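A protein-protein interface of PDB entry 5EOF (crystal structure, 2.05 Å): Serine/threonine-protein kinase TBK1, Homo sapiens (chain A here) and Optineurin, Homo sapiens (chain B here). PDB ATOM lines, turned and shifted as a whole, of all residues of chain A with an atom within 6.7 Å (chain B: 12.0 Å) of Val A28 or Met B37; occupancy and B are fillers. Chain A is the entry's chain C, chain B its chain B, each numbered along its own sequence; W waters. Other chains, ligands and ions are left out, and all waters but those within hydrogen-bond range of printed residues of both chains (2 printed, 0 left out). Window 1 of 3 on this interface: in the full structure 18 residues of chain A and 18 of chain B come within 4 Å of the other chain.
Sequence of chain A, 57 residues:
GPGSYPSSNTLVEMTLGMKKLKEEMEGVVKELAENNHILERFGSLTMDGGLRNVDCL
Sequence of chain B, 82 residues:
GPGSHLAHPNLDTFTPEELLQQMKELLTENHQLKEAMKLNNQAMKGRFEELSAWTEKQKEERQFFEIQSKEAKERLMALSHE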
ATOM      1  N   GLU A  23      24.469  19.534  26.966  1.00  0.00           N
ATOM      2  CA  GLU A  23      24.689  18.181  27.461  1.00  0.00           C
ATOM      3  C   GLU A  23      23.416  17.346  27.382  1.00  0.00           C
ATOM      4  O   GLU A  23      23.422  16.216  26.891  1.00  0.00           O
ATOM      5  CB  GLU A  23      25.143  18.226  28.916  1.00  0.00           C
ATOM      6  CG  GLU A  23      26.607  18.468  29.124  1.00  0.00           C
ATOM      7  CD  GLU A  23      26.976  18.322  30.581  1.00  0.00           C
ATOM      8  OE1 GLU A  23      27.959  18.959  31.015  1.00  0.00           O
ATOM      9  OE2 GLU A  23      26.265  17.570  31.293  1.00  0.00           O
ATOM     10  N   GLU A  24      22.329  17.911  27.882  1.00  0.00           N
ATOM     11  CA  GLU A  24      21.055  17.223  27.938  1.00  0.00           C
ATOM     12  C   GLU A  24      20.566  16.895  26.539  1.00  0.00           C
ATOM     13  O   GLU A  24      20.004  15.824  26.295  1.00  0.00           O
ATOM     14  CB  GLU A  24      20.032  18.100  28.657  1.00  0.00           C
ATOM     15  CG  GLU A  24      20.358  18.392  30.120  1.00  0.00           C
ATOM     16  CD  GLU A  24      19.484  17.608  31.075  1.00  0.00           C
ATOM     17  OE1 GLU A  24      18.783  16.689  30.611  1.00  0.00           O
ATOM     18  OE2 GLU A  24      19.489  17.898  32.287  1.00  0.00           O
ATOM     19  N   MET A  25      20.784  17.814  25.611  1.00  0.00           N
ATOM     20  CA  MET A  25      20.325  17.584  24.246  1.00  0.00           C
ATOM     21  C   MET A  25      21.138  16.487  23.568  1.00  0.00           C
ATOM     22  O   MET A  25      20.604  15.751  22.754  1.00  0.00           O
ATOM     23  CB  MET A  25      20.358  18.877  23.439  1.00  0.00           C
ATOM     24  CG  MET A  25      19.237  19.831  23.816  1.00  0.00           C
ATOM     25  SD  MET A  25      17.587  19.193  23.401  1.00  0.00           S
ATOM     26  CE  MET A  25      17.868  18.849  21.652  1.00  0.00           C
ATOM     27  N   GLU A  26      22.420  16.373  23.910  1.00  0.00           N
ATOM     28  CA  GLU A  26      23.222  15.239  23.454  1.00  0.00           C
ATOM     29  C   GLU A  26      22.540  13.932  23.867  1.00  0.00           C
ATOM     30  O   GLU A  26      22.462  12.981  23.079  1.00  0.00           O
ATOM     31  CB  GLU A  26      24.640  15.300  24.036  1.00  0.00           C
ATOM     32  CG  GLU A  26      25.572  16.292  23.346  1.00  0.00           C
ATOM     33  CD  GLU A  26      26.864  16.548  24.132  1.00  0.00           C
ATOM     34  OE1 GLU A  26      27.138  15.810  25.108  1.00  0.00           O
ATOM     35  OE2 GLU A  26      27.597  17.504  23.776  1.00  0.00           O
ATOM     36  N   GLY A  27      22.029  13.894  25.096  1.00  0.00           N
ATOM     37  CA  GLY A  27      21.353  12.710  25.592  1.00  0.00           C
ATOM     38  C   GLY A  27      20.035  12.478  24.876  1.00  0.00           C
ATOM     39  O   GLY A  27      19.724  11.359  24.481  1.00  0.00           O
ATOM     40  N   VAL A  28      19.265  13.548  24.711  1.00  0.00           N
ATOM     41  CA  VAL A  28      17.986  13.499  24.006  1.00  0.00           C
ATOM     42  C   VAL A  28      18.101  12.944  22.574  1.00  0.00           C
ATOM     43  O   VAL A  28      17.321  12.076  22.159  1.00  0.00           O
ATOM     44  CB  VAL A  28      17.356  14.902  23.965  1.00  0.00           C
ATOM     45  CG1 VAL A  28      16.149  14.915  23.059  1.00  0.00           C
ATOM     46  CG2 VAL A  28      16.972  15.353  25.370  1.00  0.00           C
ATOM     47  N   VAL A  29      19.075  13.444  21.825  1.00  0.00           N
ATOM     48  CA  VAL A  29      19.238  13.037  20.440  1.00  0.00           C
ATOM     49  C   VAL A  29      19.664  11.566  20.338  1.00  0.00           C
ATOM     50  O   VAL A  29      19.297  10.885  19.389  1.00  0.00           O
ATOM     51  CB  VAL A  29      20.195  13.968  19.668  1.00  0.00           C
ATOM     52  CG1 VAL A  29      19.724  15.422  19.780  1.00  0.00           C
ATOM     53  CG2 VAL A  29      21.578  13.861  20.213  1.00  0.00           C
ATOM     54  N   LYS A  30      20.425  11.072  21.314  1.00  0.00           N
ATOM     55  CA  LYS A  30      20.698   9.638  21.368  1.00  0.00           C
ATOM     56  C   LYS A  30      19.421   8.848  21.649  1.00  0.00           C
ATOM     57  O   LYS A  30      19.240   7.758  21.104  1.00  0.00           O
ATOM     58  CB  LYS A  30      21.768   9.307  22.406  1.00  0.00           C
ATOM     59  CG  LYS A  30      23.168   9.800  22.040  1.00  0.00           C
ATOM     60  CD  LYS A  30      24.220   9.216  22.972  1.00  0.00           C
ATOM     61  CE  LYS A  30      25.577   9.868  22.748  1.00  0.00           C
ATOM     62  NZ  LYS A  30      26.597   9.391  23.724  1.00  0.00           N
ATOM     63  N   GLU A  31      18.551   9.393  22.499  1.00  0.00           N
ATOM     64  CA  GLU A  31      17.246   8.766  22.766  1.00  0.00           C
ATOM     65  C   GLU A  31      16.435   8.690  21.483  1.00  0.00           C
ATOM     66  O   GLU A  31      15.815   7.669  21.179  1.00  0.00           O
ATOM     67  CB  GLU A  31      16.453   9.568  23.804  1.00  0.00           C
ATOM     68  CG  GLU A  31      17.090   9.638  25.191  1.00  0.00           C
ATOM     69  CD  GLU A  31      16.999   8.320  25.923  1.00  0.00           C
ATOM     70  OE1 GLU A  31      16.110   7.515  25.585  1.00  0.00           O
ATOM     71  OE2 GLU A  31      17.811   8.082  26.835  1.00  0.00           O
ATOM     72  N   LEU A  32      16.437   9.785  20.735  1.00  0.00           N
ATOM     73  CA  LEU A  32      15.753   9.838  19.452  1.00  0.00           C
ATOM     74  C   LEU A  32      16.336   8.801  18.489  1.00  0.00           C
ATOM     75  O   LEU A  32      15.590   8.127  17.796  1.00  0.00           O
ATOM     76  CB  LEU A  32      15.902  11.225  18.842  1.00  0.00           C
ATOM     77  CG  LEU A  32      14.812  11.794  17.930  1.00  0.00           C
ATOM     78  CD1 LEU A  32      15.468  12.505  16.748  1.00  0.00           C
ATOM     79  CD2 LEU A  32      13.803  10.753  17.473  1.00  0.00           C
ATOM     80  N   ALA A  33      17.666   8.704  18.436  1.00  0.00           N
ATOM     81  CA  ALA A  33      18.341   7.749  17.566  1.00  0.00           C
ATOM     82  C   ALA A  33      17.832   6.345  17.853  1.00  0.00           C
ATOM     83  O   ALA A  33      17.565   5.571  16.939  1.00  0.00           O
ATOM     84  CB  ALA A  33      19.829   7.813  17.783  1.00  0.00           C
ATOM     85  N   ASN A  35      14.906   5.539  19.304  1.00  0.00           N
ATOM     86  CA  ASN A  35      13.530   5.581  18.804  1.00  0.00           C
ATOM     87  C   ASN A  35      13.500   5.233  17.304  1.00  0.00           C
ATOM     88  O   ASN A  35      12.743   4.358  16.875  1.00  0.00           O
ATOM     89  CB  ASN A  35      12.964   6.991  19.029  1.00  0.00           C
ATOM     90  CG  ASN A  35      11.491   7.003  19.429  1.00  0.00           C
ATOM     91  OD1 ASN A  35      10.609   7.376  18.630  1.00  0.00           O
ATOM     92  ND2 ASN A  35      11.217   6.632  20.684  1.00  0.00           N
ATOM     93  N   LEU B  26      14.338  26.811  31.330  1.00  0.00           N
ATOM     94  CA  LEU B  26      14.739  25.978  30.200  1.00  0.00           C
ATOM     95  C   LEU B  26      15.404  24.696  30.667  1.00  0.00           C
ATOM     96  O   LEU B  26      15.198  23.628  30.082  1.00  0.00           O
ATOM     97  CB  LEU B  26      15.684  26.739  29.272  1.00  0.00           C
ATOM     98  CG  LEU B  26      15.011  27.819  28.427  1.00  0.00           C
ATOM     99  CD1 LEU B  26      15.996  28.358  27.402  1.00  0.00           C
ATOM    100  CD2 LEU B  26      13.759  27.260  27.741  1.00  0.00           C
ATOM    101  N   LEU B  27      16.214  24.813  31.714  1.00  0.00           N
ATOM    102  CA  LEU B  27      16.896  23.664  32.300  1.00  0.00           C
ATOM    103  C   LEU B  27      15.863  22.692  32.820  1.00  0.00           C
ATOM    104  O   LEU B  27      15.927  21.495  32.539  1.00  0.00           O
ATOM    105  CB  LEU B  27      17.816  24.113  33.440  1.00  0.00           C
ATOM    106  CG  LEU B  27      19.061  24.818  32.926  1.00  0.00           C
ATOM    107  CD1 LEU B  27      19.818  25.550  34.041  1.00  0.00           C
ATOM    108  CD2 LEU B  27      19.929  23.795  32.272  1.00  0.00           C
ATOM    109  N   THR B  28      14.898  23.219  33.564  1.00  0.00           N
ATOM    110  CA  THR B  28      13.813  22.409  34.103  1.00  0.00           C
ATOM    111  C   THR B  28      13.058  21.691  32.986  1.00  0.00           C
ATOM    112  O   THR B  28      12.871  20.461  33.029  1.00  0.00           O
ATOM    113  CB  THR B  28      12.853  23.276  34.904  1.00  0.00           C
ATOM    114  OG1 THR B  28      13.482  23.665  36.133  1.00  0.00           O
ATOM    115  CG2 THR B  28      11.583  22.521  35.208  1.00  0.00           C
ATOM    116  N   GLU B  29      12.644  22.446  31.973  1.00  0.00           N
ATOM    117  CA  GLU B  29      11.885  21.861  30.869  1.00  0.00           C
ATOM    118  C   GLU B  29      12.702  20.814  30.100  1.00  0.00           C
ATOM    119  O   GLU B  29      12.200  19.732  29.783  1.00  0.00           O
ATOM    120  CB  GLU B  29      11.387  22.964  29.926  1.00  0.00           C
ATOM    121  CG  GLU B  29      10.311  23.878  30.530  1.00  0.00           C
ATOM    122  CD  GLU B  29       9.692  24.809  29.490  1.00  0.00           C
ATOM    123  OE1 GLU B  29      10.196  24.840  28.342  1.00  0.00           O
ATOM    124  OE2 GLU B  29       8.703  25.504  29.816  1.00  0.00           O
ATOM    125  N   ASN B  30      13.954  21.144  29.796  1.00  0.00           N
ATOM    126  CA  ASN B  30      14.841  20.224  29.084  1.00  0.00           C
ATOM    127  C   ASN B  30      15.064  18.932  29.862  1.00  0.00           C
ATOM    128  O   ASN B  30      15.027  17.836  29.287  1.00  0.00           O
ATOM    129  CB  ASN B  30      16.183  20.880  28.772  1.00  0.00           C
ATOM    130  CG  ASN B  30      16.778  20.394  27.470  1.00  0.00           C
ATOM    131  OD1 ASN B  30      16.597  21.004  26.415  1.00  0.00           O
ATOM    132  ND2 ASN B  30      17.480  19.285  27.533  1.00  0.00           N
ATOM    133  N   HIS B  31      15.285  19.057  31.171  1.00  0.00           N
ATOM    134  CA  HIS B  31      15.468  17.877  31.999  1.00  0.00           C
ATOM    135  C   HIS B  31      14.207  17.009  31.954  1.00  0.00           C
ATOM    136  O   HIS B  31      14.284  15.775  31.844  1.00  0.00           O
ATOM    137  CB  HIS B  31      15.794  18.248  33.440  1.00  0.00           C
ATOM    138  CG  HIS B  31      16.180  17.068  34.275  1.00  0.00           C
ATOM    139  ND1 HIS B  31      17.400  16.439  34.151  1.00  0.00           N
ATOM    140  CD2 HIS B  31      15.493  16.379  35.217  1.00  0.00           C
ATOM    141  CE1 HIS B  31      17.455  15.421  34.994  1.00  0.00           C
ATOM    142  NE2 HIS B  31      16.311  15.363  35.651  1.00  0.00           N
ATOM    143  N   GLN B  32      13.053  17.667  32.046  1.00  0.00           N
ATOM    144  CA  GLN B  32      11.758  17.007  31.961  1.00  0.00           C
ATOM    145  C   GLN B  32      11.637  16.242  30.646  1.00  0.00           C
ATOM    146  O   GLN B  32      11.241  15.079  30.638  1.00  0.00           O
ATOM    147  CB  GLN B  32      10.654  18.054  32.052  1.00  0.00           C
ATOM    148  CG  GLN B  32       9.474  17.664  32.924  1.00  0.00           C
ATOM    149  CD  GLN B  32       8.403  18.747  32.967  1.00  0.00           C
ATOM    150  OE1 GLN B  32       8.710  19.939  32.921  1.00  0.00           O
ATOM    151  NE2 GLN B  32       7.137  18.332  33.038  1.00  0.00           N
ATOM    152  N   LEU B  33      11.971  16.913  29.543  1.00  0.00           N
ATOM    153  CA  LEU B  33      11.969  16.298  28.221  1.00  0.00           C
ATOM    154  C   LEU B  33      12.861  15.072  28.181  1.00  0.00           C
ATOM    155  O   LEU B  33      12.475  14.035  27.624  1.00  0.00           O
ATOM    156  CB  LEU B  33      12.415  17.289  27.145  1.00  0.00           C
ATOM    157  CG  LEU B  33      12.514  16.713  25.729  1.00  0.00           C
ATOM    158  CD1 LEU B  33      11.131  16.400  25.180  1.00  0.00           C
ATOM    159  CD2 LEU B  33      13.276  17.651  24.792  1.00  0.00           C
ATOM    160  N   LYS B  34      14.045  15.170  28.780  1.00  0.00           N
ATOM    161  CA  LYS B  34      14.981  14.052  28.684  1.00  0.00           C
ATOM    162  C   LYS B  34      14.433  12.817  29.385  1.00  0.00           C
ATOM    163  O   LYS B  34      14.524  11.693  28.859  1.00  0.00           O
ATOM    164  CB  LYS B  34      16.365  14.400  29.242  1.00  0.00           C
ATOM    165  CG  LYS B  34      17.405  13.301  28.958  1.00  0.00           C
ATOM    166  CD  LYS B  34      18.730  13.538  29.682  1.00  0.00           C
ATOM    167  CE  LYS B  34      18.552  13.496  31.197  1.00  0.00           C
ATOM    168  NZ  LYS B  34      19.812  13.806  31.950  1.00  0.00           N
ATOM    169  N   GLU B  35      13.871  13.027  30.572  1.00  0.00           N
ATOM    170  CA  GLU B  35      13.332  11.919  31.352  1.00  0.00           C
ATOM    171  C   GLU B  35      12.112  11.314  30.658  1.00  0.00           C
ATOM    172  O   GLU B  35      11.950  10.086  30.629  1.00  0.00           O
ATOM    173  CB  GLU B  35      12.998  12.363  32.776  1.00  0.00           C
ATOM    174  CG  GLU B  35      14.233  12.724  33.605  1.00  0.00           C
ATOM    175  CD  GLU B  35      15.253  11.591  33.660  1.00  0.00           C
ATOM    176  OE1 GLU B  35      14.897  10.481  34.125  1.00  0.00           O
ATOM    177  OE2 GLU B  35      16.411  11.810  33.233  1.00  0.00           O
ATOM    178  N   ALA B  36      11.282  12.172  30.069  1.00  0.00           N
ATOM    179  CA  ALA B  36      10.119  11.703  29.307  1.00  0.00           C
ATOM    180  C   ALA B  36      10.552  10.862  28.100  1.00  0.00           C
ATOM    181  O   ALA B  36       9.925   9.840  27.758  1.00  0.00           O
ATOM    182  CB  ALA B  36       9.284  12.873  28.859  1.00  0.00           C
ATOM    183  N   MET B  37      11.626  11.299  27.445  1.00  0.00           N
ATOM    184  CA  MET B  37      12.139  10.574  26.294  1.00  0.00           C
ATOM    185  C   MET B  37      12.643   9.185  26.685  1.00  0.00           C
ATOM    186  O   MET B  37      12.406   8.211  25.965  1.00  0.00           O
ATOM    187  CB  MET B  37      13.228  11.376  25.593  1.00  0.00           C
ATOM    188  CG  MET B  37      12.931  11.606  24.131  1.00  0.00           C
ATOM    189  SD  MET B  37      13.235  13.306  23.630  1.00  0.00           S
ATOM    190  CE  MET B  37      13.145  13.127  21.849  1.00  0.00           C
ATOM    191  N   LYS B  38      13.322   9.088  27.827  1.00  0.00           N
ATOM    192  CA  LYS B  38      13.769   7.787  28.333  1.00  0.00           C
ATOM    193  C   LYS B  38      12.578   6.880  28.581  1.00  0.00           C
ATOM    194  O   LYS B  38      12.600   5.684  28.248  1.00  0.00           O
ATOM    195  CB  LYS B  38      14.528   7.937  29.647  1.00  0.00           C
ATOM    196  CG  LYS B  38      15.850   8.665  29.558  1.00  0.00           C
ATOM    197  CD  LYS B  38      16.722   8.284  30.752  1.00  0.00           C
ATOM    198  CE  LYS B  38      17.911   9.219  30.911  1.00  0.00           C
ATOM    199  NZ  LYS B  38      17.486  10.506  31.522  1.00  0.00           N
ATOM    200  N   LEU B  39      11.540   7.448  29.191  1.00  0.00           N
ATOM    201  CA  LEU B  39      10.304   6.698  29.438  1.00  0.00           C
ATOM    202  C   LEU B  39       9.675   6.275  28.124  1.00  0.00           C
ATOM    203  O   LEU B  39       9.211   5.154  27.987  1.00  0.00           O
ATOM    204  CB  LEU B  39       9.310   7.554  30.221  1.00  0.00           C
ATOM    205  CG  LEU B  39       9.037   7.134  31.665  1.00  0.00           C
ATOM    206  CD1 LEU B  39      10.293   6.606  32.343  1.00  0.00           C
ATOM    207  CD2 LEU B  39       8.478   8.310  32.438  1.00  0.00           C
ATOM    208  N   ASN B  40       9.677   7.185  27.154  1.00  0.00           N
ATOM    209  CA  ASN B  40       9.075   6.923  25.862  1.00  0.00           C
ATOM    210  C   ASN B  40       9.813   5.822  25.122  1.00  0.00           C
ATOM    211  O   ASN B  40       9.203   5.008  24.456  1.00  0.00           O
ATOM    212  CB  ASN B  40       9.024   8.193  25.020  1.00  0.00           C
ATOM    213  CG  ASN B  40       8.631   7.927  23.588  1.00  0.00           C
ATOM    214  OD1 ASN B  40       9.486   7.850  22.717  1.00  0.00           O
ATOM    215  ND2 ASN B  40       7.333   7.783  23.335  1.00  0.00           N
ATOM    216  N   ASN B  41      11.132   5.808  25.239  1.00  0.00           N
ATOM    217  CA  ASN B  41      11.884   4.756  24.584  1.00  0.00           C
ATOM    218  C   ASN B  41      11.730   3.407  25.271  1.00  0.00           C
ATOM    219  O   ASN B  41      11.717   2.370  24.596  1.00  0.00           O
ATOM    220  CB  ASN B  41      13.344   5.147  24.379  1.00  0.00           C
ATOM    221  CG  ASN B  41      13.565   5.870  23.057  1.00  0.00           C
ATOM    222  OD1 ASN B  41      13.088   5.434  21.992  1.00  0.00           O
ATOM    223  ND2 ASN B  41      14.285   6.974  23.115  1.00  0.00           N
ATOM    224  N   GLN B  42      11.552   3.407  26.585  1.00  0.00           N
ATOM    225  CA  GLN B  42      11.234   2.170  27.291  1.00  0.00           C
ATOM    226  C   GLN B  42       9.896   1.639  26.777  1.00  0.00           C
ATOM    227  O   GLN B  42       9.733   0.429  26.529  1.00  0.00           O
ATOM    228  CB  GLN B  42      11.181   2.424  28.801  1.00  0.00           C
ATOM    229  CG  GLN B  42      10.825   1.209  29.642  1.00  0.00           C
ATOM    230  CD  GLN B  42      10.779   1.524  31.131  1.00  0.00           C
ATOM    231  OE1 GLN B  42      10.909   2.683  31.540  1.00  0.00           O
ATOM    232  NE2 GLN B  42      10.594   0.491  31.948  1.00  0.00           N
ATOM    233  N   ALA B  43       8.941   2.543  26.576  1.00  0.00           N
ATOM    234  CA  ALA B  43       7.634   2.141  26.044  1.00  0.00           C
ATOM    235  C   ALA B  43       7.735   1.597  24.618  1.00  0.00           C
ATOM    236  O   ALA B  43       7.071   0.607  24.285  1.00  0.00           O
ATOM    237  CB  ALA B  43       6.640   3.280  26.111  1.00  0.00           C
ATOM    238  N   MET B  44       8.554   2.239  23.781  1.00  0.00           N
ATOM    239  CA  MET B  44       8.767   1.775  22.405  1.00  0.00           C
ATOM    240  C   MET B  44       9.248   0.336  22.407  1.00  0.00           C
ATOM    241  O   MET B  44       8.773  -0.510  21.630  1.00  0.00           O
ATOM    242  CB  MET B  44       9.818   2.624  21.691  1.00  0.00           C
ATOM    243  CG  MET B  44       9.280   3.871  21.005  1.00  0.00           C
ATOM    244  SD  MET B  44       8.347   3.507  19.506  1.00  0.00           S
ATOM    245  CE  MET B  44       9.665   3.118  18.357  1.00  0.00           C
ATOM    246  N   LYS B  45      10.200   0.066  23.290  1.00  0.00           N
ATOM    247  CA  LYS B  45      10.848  -1.240  23.365  1.00  0.00           C
ATOM    248  C   LYS B  45       9.865  -2.287  23.895  1.00  0.00           C
ATOM    249  O   LYS B  45       9.831  -3.419  23.411  1.00  0.00           O
ATOM    250  CB  LYS B  45      12.102  -1.137  24.248  1.00  0.00           C
ATOM    251  CG  LYS B  45      12.887  -2.425  24.405  1.00  0.00           C
ATOM    252  CD  LYS B  45      14.294  -2.158  24.952  1.00  0.00           C
ATOM    253  CE  LYS B  45      15.117  -3.462  25.053  1.00  0.00           C
ATOM    254  NZ  LYS B  45      15.252  -4.003  26.449  1.00  0.00           N
ATOM    255  N   GLY B  46       9.069  -1.896  24.892  1.00  0.00           N
ATOM    256  CA  GLY B  46       8.059  -2.764  25.465  1.00  0.00           C
ATOM    257  C   GLY B  46       7.001  -3.126  24.439  1.00  0.00           C
ATOM    258  O   GLY B  46       6.633  -4.301  24.303  1.00  0.00           O
HETATM  259  O   HOH W   1      18.598  20.539  32.744  1.00  0.00           O
HETATM  260  O   HOH W   2       8.247   6.524  17.415  1.00  0.00           O
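The side-chain amide oxygen (OD1) of Asn B40 sits at hydrogen-bond distance from the side-chain amide nitrogen (ND2) of Asn A35. NZ of Lys B34 lies within salt-bridge range of OE1 of Glu A24, 3.3 Å away. The side-chain amide oxygen of Asn B41 lies within hydrogen-bond range of the side-chain amide nitrogen of Asn A35 (2.6 Å). The side-chain carboxylate (OE2) of Glu A24 sits at hydrogen-bond distance from a ring nitrogen (ND1) of His B31, 3.2 Å away. The side-chain sulfur (SD) of Met A25 sits close to the side-chain amide oxygen (OD1) of Asn B30, 3.7 Å away. The backbone carbonyl oxygen (O) of Glu A31 is in hydrogen-bond range of the side-chain amide nitrogen (ND2) of Asn B41, at 2.6 Å.
Of chain B, only Asn B30, His B31 and Lys B34 come within 4 Å of Glu A24. No residue of chain B comes within 4 Å of Gly A27. Of the printed residues of chain B, Val A28 touches Met B37 (3.4 Å). Of the printed residues of chain B, Asn A35 touches Asn B40, Asn B41 and Met B44. Printed residues of chain A within 4 Å of Asn B30: Glu A24 and Met A25. Printed residues of chain A within 4 Å of Lys B34: Glu A24 (3.3 Å). Ala B36 touches none of the printed residues of chain A. Leu B39 touches none of the printed residues of chain A. Of the printed residues of chain A, Asn B40 touches Asn A35. Printed residues of chain A within 4 Å of Asn B41: Glu A31 and Asn A35.
Of the 21 printed residues of chain B, 8 touch a printed residue of chain A. Along chain A the printed residues that touch a printed residue of chain B span positions 24 to 35. Among the printed residues, 11 pairs touch across the chains. Among the printed residues, Asp or Glu carboxylates within 4 Å of a Lys or Arg side-chain nitrogen of the other chain: Glu A24 with Lys B34.
NZ of Lys B38 is in salt-bridge range of OE2 of Glu B35 (2.4 Å).
Water W2 lies within hydrogen-bond range of OD1 of Asn A35 (2.8 Å) and SD of Met B44 (3.7 Å). Water W1 bridges the side-chain carboxylate of Glu A24 (2.8 Å) and the backbone carbonyl oxygen of Leu B27 (2.8 Å).
Asn B30 touches Glu A24 (ND2 to CB, 3.0 Å). SD of Met B37 touches CG1 of Val A28, at 3.4 Å. O of Met B37 touches OE1 of Glu A31, at 3.8 Å. Glu A31 touches Lys B38 (OE2 to CG, 3.4 Å). Asn A35 touches Met B44.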
